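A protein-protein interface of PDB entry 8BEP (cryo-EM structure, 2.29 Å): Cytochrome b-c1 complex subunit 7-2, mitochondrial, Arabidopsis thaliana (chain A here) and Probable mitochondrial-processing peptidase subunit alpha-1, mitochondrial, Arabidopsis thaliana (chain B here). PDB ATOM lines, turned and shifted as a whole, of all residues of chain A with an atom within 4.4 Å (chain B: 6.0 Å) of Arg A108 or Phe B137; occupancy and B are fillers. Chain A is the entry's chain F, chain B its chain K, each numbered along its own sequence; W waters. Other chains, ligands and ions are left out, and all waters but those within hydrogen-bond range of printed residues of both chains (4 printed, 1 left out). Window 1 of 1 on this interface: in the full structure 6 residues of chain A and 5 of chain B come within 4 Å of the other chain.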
ATOM      1  N   GLU A 104     -28.346 -15.838  20.148  1.00  0.00           N
ATOM      2  CA  GLU A 104     -27.582 -15.058  19.178  1.00  0.00           C
ATOM      3  C   GLU A 104     -27.375 -15.830  17.877  1.00  0.00           C
ATOM      4  O   GLU A 104     -27.484 -15.261  16.782  1.00  0.00           O
ATOM      5  CB  GLU A 104     -26.245 -14.639  19.788  1.00  0.00           C
ATOM      6  CG  GLU A 104     -26.390 -13.627  20.918  1.00  0.00           C
ATOM      7  CD  GLU A 104     -25.065 -13.261  21.559  1.00  0.00           C
ATOM      8  OE1 GLU A 104     -25.020 -12.265  22.309  1.00  0.00           O
ATOM      9  OE2 GLU A 104     -24.072 -13.974  21.316  1.00  0.00           O
ATOM     10  N   ARG A 105     -27.084 -17.130  17.973  1.00  0.00           N
ATOM     11  CA  ARG A 105     -26.931 -17.932  16.761  1.00  0.00           C
ATOM     12  C   ARG A 105     -28.243 -18.039  15.993  1.00  0.00           C
ATOM     13  O   ARG A 105     -28.251 -17.992  14.757  1.00  0.00           O
ATOM     14  CB  ARG A 105     -26.391 -19.322  17.096  1.00  0.00           C
ATOM     15  CG  ARG A 105     -24.883 -19.455  16.933  1.00  0.00           C
ATOM     16  CD  ARG A 105     -24.391 -19.178  15.494  1.00  0.00           C
ATOM     17  NE  ARG A 105     -25.345 -19.555  14.453  1.00  0.00           N
ATOM     18  CZ  ARG A 105     -25.499 -20.788  13.989  1.00  0.00           C
ATOM     19  NH1 ARG A 105     -24.785 -21.798  14.457  1.00  0.00           N
ATOM     20  NH2 ARG A 105     -26.392 -21.013  13.028  1.00  0.00           N
ATOM     21  N   ALA A 106     -29.364 -18.187  16.707  1.00  0.00           N
ATOM     22  CA  ALA A 106     -30.661 -18.217  16.039  1.00  0.00           C
ATOM     23  C   ALA A 106     -30.944 -16.898  15.333  1.00  0.00           C
ATOM     24  O   ALA A 106     -31.483 -16.885  14.220  1.00  0.00           O
ATOM     25  CB  ALA A 106     -31.768 -18.540  17.042  1.00  0.00           C
ATOM     26  N   GLU A 107     -30.584 -15.780  15.963  1.00  0.00           N
ATOM     27  CA  GLU A 107     -30.759 -14.484  15.318  1.00  0.00           C
ATOM     28  C   GLU A 107     -29.925 -14.388  14.045  1.00  0.00           C
ATOM     29  O   GLU A 107     -30.407 -13.908  13.015  1.00  0.00           O
ATOM     30  CB  GLU A 107     -30.394 -13.357  16.283  1.00  0.00           C
ATOM     31  CG  GLU A 107     -30.779 -11.974  15.783  1.00  0.00           C
ATOM     32  CD  GLU A 107     -30.194 -10.849  16.620  1.00  0.00           C
ATOM     33  OE1 GLU A 107     -29.172 -11.067  17.303  1.00  0.00           O
ATOM     34  OE2 GLU A 107     -30.763  -9.741  16.597  1.00  0.00           O
ATOM     35  N   ARG A 108     -28.673 -14.852  14.099  1.00  0.00           N
ATOM     36  CA  ARG A 108     -27.823 -14.824  12.912  1.00  0.00           C
ATOM     37  C   ARG A 108     -28.406 -15.670  11.788  1.00  0.00           C
ATOM     38  O   ARG A 108     -28.404 -15.257  10.624  1.00  0.00           O
ATOM     39  CB  ARG A 108     -26.416 -15.303  13.257  1.00  0.00           C
ATOM     40  CG  ARG A 108     -25.652 -14.378  14.170  1.00  0.00           C
ATOM     41  CD  ARG A 108     -24.168 -14.664  14.133  1.00  0.00           C
ATOM     42  NE  ARG A 108     -23.602 -14.500  12.800  1.00  0.00           N
ATOM     43  CZ  ARG A 108     -22.925 -13.430  12.411  1.00  0.00           C
ATOM     44  NH1 ARG A 108     -22.749 -12.394  13.214  1.00  0.00           N
ATOM     45  NH2 ARG A 108     -22.417 -13.396  11.185  1.00  0.00           N
ATOM     46  N   GLU A 109     -28.907 -16.863  12.118  1.00  0.00           N
ATOM     47  CA  GLU A 109     -29.477 -17.731  11.091  1.00  0.00           C
ATOM     48  C   GLU A 109     -30.751 -17.135  10.503  1.00  0.00           C
ATOM     49  O   GLU A 109     -30.988 -17.234   9.294  1.00  0.00           O
ATOM     50  CB  GLU A 109     -29.743 -19.122  11.663  1.00  0.00           C
ATOM     51  CG  GLU A 109     -30.248 -20.136  10.654  1.00  0.00           C
ATOM     52  CD  GLU A 109     -29.428 -20.160   9.374  1.00  0.00           C
ATOM     53  OE1 GLU A 109     -28.319 -20.733   9.389  1.00  0.00           O
ATOM     54  OE2 GLU A 109     -29.896 -19.617   8.351  1.00  0.00           O
ATOM     55  N   ALA A 110     -31.578 -16.502  11.339  1.00  0.00           N
ATOM     56  CA  ALA A 110     -32.831 -15.926  10.868  1.00  0.00           C
ATOM     57  C   ALA A 110     -32.623 -14.753   9.916  1.00  0.00           C
ATOM     58  O   ALA A 110     -33.534 -14.427   9.150  1.00  0.00           O
ATOM     59  CB  ALA A 110     -33.679 -15.478  12.057  1.00  0.00           C
ATOM     60  N   LEU A 111     -31.460 -14.107   9.948  1.00  0.00           N
ATOM     61  CA  LEU A 111     -31.170 -12.993   9.059  1.00  0.00           C
ATOM     62  C   LEU A 111     -30.258 -13.385   7.901  1.00  0.00           C
ATOM     63  O   LEU A 111     -29.836 -12.513   7.138  1.00  0.00           O
ATOM     64  CB  LEU A 111     -30.558 -11.836   9.849  1.00  0.00           C
ATOM     65  CG  LEU A 111     -31.507 -11.050  10.758  1.00  0.00           C
ATOM     66  CD1 LEU A 111     -30.846  -9.778  11.250  1.00  0.00           C
ATOM     67  CD2 LEU A 111     -32.799 -10.728  10.040  1.00  0.00           C
ATOM     68  N   GLY A 112     -29.949 -14.671   7.753  1.00  0.00           N
ATOM     69  CA  GLY A 112     -29.151 -15.132   6.634  1.00  0.00           C
ATOM     70  C   GLY A 112     -27.662 -14.904   6.751  1.00  0.00           C
ATOM     71  O   GLY A 112     -26.963 -14.939   5.736  1.00  0.00           O
ATOM     72  N   ALA A 113     -27.154 -14.674   7.956  1.00  0.00           N
ATOM     73  CA  ALA A 113     -25.738 -14.420   8.159  1.00  0.00           C
ATOM     74  C   ALA A 113     -24.952 -15.726   8.247  1.00  0.00           C
ATOM     75  O   ALA A 113     -25.500 -16.803   8.487  1.00  0.00           O
ATOM     76  CB  ALA A 113     -25.520 -13.595   9.427  1.00  0.00           C
ATOM     77  N   LEU A 114     -23.647 -15.613   8.044  1.00  0.00           N
ATOM     78  CA  LEU A 114     -22.762 -16.749   8.240  1.00  0.00           C
ATOM     79  C   LEU A 114     -22.613 -17.039   9.733  1.00  0.00           C
ATOM     80  O   LEU A 114     -22.583 -16.111  10.544  1.00  0.00           O
ATOM     81  CB  LEU A 114     -21.393 -16.469   7.623  1.00  0.00           C
ATOM     82  CG  LEU A 114     -21.293 -16.436   6.094  1.00  0.00           C
ATOM     83  CD1 LEU A 114     -19.871 -16.727   5.649  1.00  0.00           C
ATOM     84  CD2 LEU A 114     -22.261 -17.429   5.464  1.00  0.00           C
ATOM     85  N   LEU A 116     -20.907 -17.719  13.296  1.00  0.00           N
ATOM     86  CA  LEU A 116     -19.685 -17.175  13.876  1.00  0.00           C
ATOM     87  C   LEU A 116     -18.626 -18.242  14.115  1.00  0.00           C
ATOM     88  O   LEU A 116     -17.444 -17.908  14.238  1.00  0.00           O
ATOM     89  CB  LEU A 116     -20.004 -16.462  15.187  1.00  0.00           C
ATOM     90  CG  LEU A 116     -20.534 -15.030  15.076  1.00  0.00           C
ATOM     91  CD1 LEU A 116     -20.626 -14.397  16.448  1.00  0.00           C
ATOM     92  CD2 LEU A 116     -19.663 -14.194  14.150  1.00  0.00           C
ATOM     93  N   SER B 130     -23.025  -3.618  20.991  1.00  0.00           N
ATOM     94  CA  SER B 130     -24.271  -4.111  21.566  1.00  0.00           C
ATOM     95  C   SER B 130     -24.816  -3.143  22.611  1.00  0.00           C
ATOM     96  O   SER B 130     -24.065  -2.553  23.389  1.00  0.00           O
ATOM     97  CB  SER B 130     -24.058  -5.486  22.204  1.00  0.00           C
ATOM     98  OG  SER B 130     -23.481  -6.407  21.301  1.00  0.00           O
ATOM     99  N   THR B 135     -28.473  -6.508  19.871  1.00  0.00           N
ATOM    100  CA  THR B 135     -27.115  -7.001  19.729  1.00  0.00           C
ATOM    101  C   THR B 135     -26.345  -6.147  18.732  1.00  0.00           C
ATOM    102  O   THR B 135     -26.925  -5.397  17.943  1.00  0.00           O
ATOM    103  CB  THR B 135     -27.119  -8.458  19.265  1.00  0.00           C
ATOM    104  OG1 THR B 135     -27.777  -8.553  17.998  1.00  0.00           O
ATOM    105  CG2 THR B 135     -27.849  -9.330  20.274  1.00  0.00           C
ATOM    106  N   HIS B 136     -25.020  -6.267  18.780  1.00  0.00           N
ATOM    107  CA  HIS B 136     -24.171  -5.624  17.785  1.00  0.00           C
ATOM    108  C   HIS B 136     -24.557  -6.064  16.375  1.00  0.00           C
ATOM    109  O   HIS B 136     -24.606  -5.251  15.444  1.00  0.00           O
ATOM    110  CB  HIS B 136     -22.707  -5.948  18.091  1.00  0.00           C
ATOM    111  CG  HIS B 136     -21.725  -5.239  17.211  1.00  0.00           C
ATOM    112  ND1 HIS B 136     -20.407  -5.629  17.108  1.00  0.00           N
ATOM    113  CD2 HIS B 136     -21.864  -4.167  16.397  1.00  0.00           C
ATOM    114  CE1 HIS B 136     -19.778  -4.829  16.269  1.00  0.00           C
ATOM    115  NE2 HIS B 136     -20.640  -3.934  15.823  1.00  0.00           N
ATOM    116  N   PHE B 137     -24.859  -7.354  16.210  1.00  0.00           N
ATOM    117  CA  PHE B 137     -25.238  -7.878  14.904  1.00  0.00           C
ATOM    118  C   PHE B 137     -26.502  -7.205  14.380  1.00  0.00           C
ATOM    119  O   PHE B 137     -26.557  -6.771  13.223  1.00  0.00           O
ATOM    120  CB  PHE B 137     -25.425  -9.396  14.991  1.00  0.00           C
ATOM    121  CG  PHE B 137     -26.056  -9.999  13.773  1.00  0.00           C
ATOM    122  CD1 PHE B 137     -25.338 -10.121  12.593  1.00  0.00           C
ATOM    123  CD2 PHE B 137     -27.366 -10.440  13.805  1.00  0.00           C
ATOM    124  CE1 PHE B 137     -25.917 -10.671  11.468  1.00  0.00           C
ATOM    125  CE2 PHE B 137     -27.948 -10.996  12.687  1.00  0.00           C
ATOM    126  CZ  PHE B 137     -27.223 -11.109  11.512  1.00  0.00           C
ATOM    127  N   ARG B 138     -27.523  -7.087  15.229  1.00  0.00           N
ATOM    128  CA  ARG B 138     -28.765  -6.469  14.784  1.00  0.00           C
ATOM    129  C   ARG B 138     -28.578  -4.979  14.522  1.00  0.00           C
ATOM    130  O   ARG B 138     -29.194  -4.427  13.608  1.00  0.00           O
ATOM    131  CB  ARG B 138     -29.877  -6.712  15.802  1.00  0.00           C
ATOM    132  CG  ARG B 138     -31.171  -6.007  15.447  1.00  0.00           C
ATOM    133  CD  ARG B 138     -32.209  -6.103  16.537  1.00  0.00           C
ATOM    134  NE  ARG B 138     -33.217  -5.062  16.398  1.00  0.00           N
ATOM    135  CZ  ARG B 138     -34.473  -5.278  16.031  1.00  0.00           C
ATOM    136  NH1 ARG B 138     -34.910  -6.493  15.750  1.00  0.00           N
ATOM    137  NH2 ARG B 138     -35.307  -4.247  15.938  1.00  0.00           N
ATOM    138  N   LEU B 139     -27.721  -4.316  15.299  1.00  0.00           N
ATOM    139  CA  LEU B 139     -27.431  -2.906  15.055  1.00  0.00           C
ATOM    140  C   LEU B 139     -26.785  -2.704  13.687  1.00  0.00           C
ATOM    141  O   LEU B 139     -27.202  -1.836  12.907  1.00  0.00           O
ATOM    142  CB  LEU B 139     -26.527  -2.369  16.162  1.00  0.00           C
ATOM    143  CG  LEU B 139     -26.346  -0.858  16.255  1.00  0.00           C
ATOM    144  CD1 LEU B 139     -27.692  -0.189  16.402  1.00  0.00           C
ATOM    145  CD2 LEU B 139     -25.455  -0.514  17.429  1.00  0.00           C
ATOM    146  N   VAL B 140     -25.763  -3.508  13.382  1.00  0.00           N
ATOM    147  CA  VAL B 140     -25.102  -3.410  12.086  1.00  0.00           C
ATOM    148  C   VAL B 140     -26.089  -3.692  10.964  1.00  0.00           C
ATOM    149  O   VAL B 140     -26.106  -2.992   9.945  1.00  0.00           O
ATOM    150  CB  VAL B 140     -23.884  -4.350  12.029  1.00  0.00           C
ATOM    151  CG1 VAL B 140     -23.326  -4.429  10.609  1.00  0.00           C
ATOM    152  CG2 VAL B 140     -22.811  -3.882  12.993  1.00  0.00           C
ATOM    153  N   ARG B 141     -26.940  -4.707  11.135  1.00  0.00           N
ATOM    154  CA  ARG B 141     -27.905  -5.026  10.088  1.00  0.00           C
ATOM    155  C   ARG B 141     -28.933  -3.912   9.913  1.00  0.00           C
ATOM    156  O   ARG B 141     -29.335  -3.610   8.785  1.00  0.00           O
ATOM    157  CB  ARG B 141     -28.577  -6.365  10.383  1.00  0.00           C
ATOM    158  CG  ARG B 141     -27.693  -7.560  10.053  1.00  0.00           C
ATOM    159  CD  ARG B 141     -27.116  -7.443   8.648  1.00  0.00           C
ATOM    160  NE  ARG B 141     -26.131  -8.477   8.357  1.00  0.00           N
ATOM    161  CZ  ARG B 141     -26.421  -9.667   7.849  1.00  0.00           C
ATOM    162  NH1 ARG B 141     -27.666 -10.018   7.580  1.00  0.00           N
ATOM    163  NH2 ARG B 141     -25.437 -10.524   7.604  1.00  0.00           N
ATOM    164  N   GLU B 142     -29.362  -3.283  11.012  1.00  0.00           N
ATOM    165  CA  GLU B 142     -30.297  -2.169  10.915  1.00  0.00           C
ATOM    166  C   GLU B 142     -29.685  -1.000  10.155  1.00  0.00           C
ATOM    167  O   GLU B 142     -30.339  -0.400   9.297  1.00  0.00           O
ATOM    168  CB  GLU B 142     -30.736  -1.716  12.309  1.00  0.00           C
ATOM    169  CG  GLU B 142     -31.792  -2.591  12.962  1.00  0.00           C
ATOM    170  CD  GLU B 142     -31.827  -2.439  14.472  1.00  0.00           C
ATOM    171  OE1 GLU B 142     -30.776  -2.125  15.069  1.00  0.00           O
ATOM    172  OE2 GLU B 142     -32.907  -2.638  15.065  1.00  0.00           O
HETATM  173  O   HOH W   1     -29.180 -11.439   4.874  1.00  0.00           O
HETATM  174  O   HOH W   2     -23.379 -11.184   9.613  1.00  0.00           O
HETATM  175  O   HOH W   3     -26.121 -12.184   4.962  1.00  0.00           O
HETATM  176  O   HOH W   4     -30.927  -8.196  19.059  1.00  0.00           O
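The side-chain hydroxyl (OG1) of Thr B135 lies within hydrogen-bond range of the side-chain carboxylate (OE1) of Glu A107, at 3.0 Å.
The backbone carbonyl oxygen (O) of Leu A111 is in hydrogen-bond range of the guanidinium group (NH1) of Arg B141, at 3.3 Å.
The side-chain hydroxyl (OG1) of Thr B135 sits at hydrogen-bond distance from the backbone NH (N) of Arg B138 (3.1 Å).
The guanidinium group (NE) of Arg B138 is in salt-bridge range of the side-chain carboxylate (OE2) of Glu B142 (2.8 Å).
The backbone carbonyl oxygen (O) of Arg A108 lies within hydrogen-bond range of the backbone NH (N) of Ala A113, at 3.0 Å.
The guanidinium group (NH2) of Arg A108 lies within hydrogen-bond range of the backbone carbonyl oxygen (O) of Leu A114.
Among the printed residues, merely in contact across the chains: Glu A107 with Phe B137 (3.8 Å), Glu A107 with Arg B138 (3.3 Å), Arg A108 with Phe B137 (3.5 Å), Leu A111 with Phe B137 (3.5 Å), Ala A113 with Phe B137 (3.6 Å) and Ala A113 with Arg B141 (3.6 Å).
Of the printed residues of chain B, Glu A107 touches Thr B135, Phe B137 and Arg B138.
Arg A108 touches just one residue of chain B: Phe B137 (3.5 Å).
Of the printed residues of chain B, Ala A113 touches Phe B137 and Arg B141.
Phe B137 touches just these residues of chain A: Glu A107 (3.8 Å), Arg A108 (3.5 Å), Leu A111 (3.5 Å) and Ala A113 (3.6 Å).
Printed residues of chain A within 4 Å of Arg B138: Glu A107 (3.3 Å).
Val B140 touches none of the printed residues of chain A.
Printed residues of chain A within 4 Å of Arg B141: Leu A111 (3.3 Å) and Ala A113 (3.6 Å).
The nearest residue of chain B that does not touch Arg A108 is Arg B141 (5.5 Å).
The nearest printed residue of chain A that does not touch Phe B137 is Glu A104 (5.7 Å).
Of the 9 printed residues of chain B, 4 touch a printed residue of chain A.
Of the 12 printed residues of chain A, 4 touch a printed residue of chain B.
Hydrophobic or aromatic side chains of chain A within 4 Å of the printed part of chain B: Leu A111 and Ala A113.
Along chain A the printed residues that touch a printed residue of chain B span positions 107 to 113.
Among the printed residues, 8 pairs touch across the chains.
Among the printed residues, no Asp or Glu carboxylate lies within 4 Å of a Lys or Arg side-chain nitrogen of the other chain.
Water W1 lies within hydrogen-bond range of O of Leu A111 (2.6 Å) and NH1 of Arg B141 (3.4 Å).
Water W2 bridges NH2 of Arg A108 (2.9 Å) and NH2 of Arg B141 (3.0 Å).
Water W4 lies within hydrogen-bond range of OE2 of Glu A107 (2.9 Å) and N of Thr B135 (3.1 Å).
Water W3 lies within hydrogen-bond range of the backbone carbonyl oxygen of Gly A112 (3.0 Å) and the guanidinium group of Arg B141 (3.2 Å).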
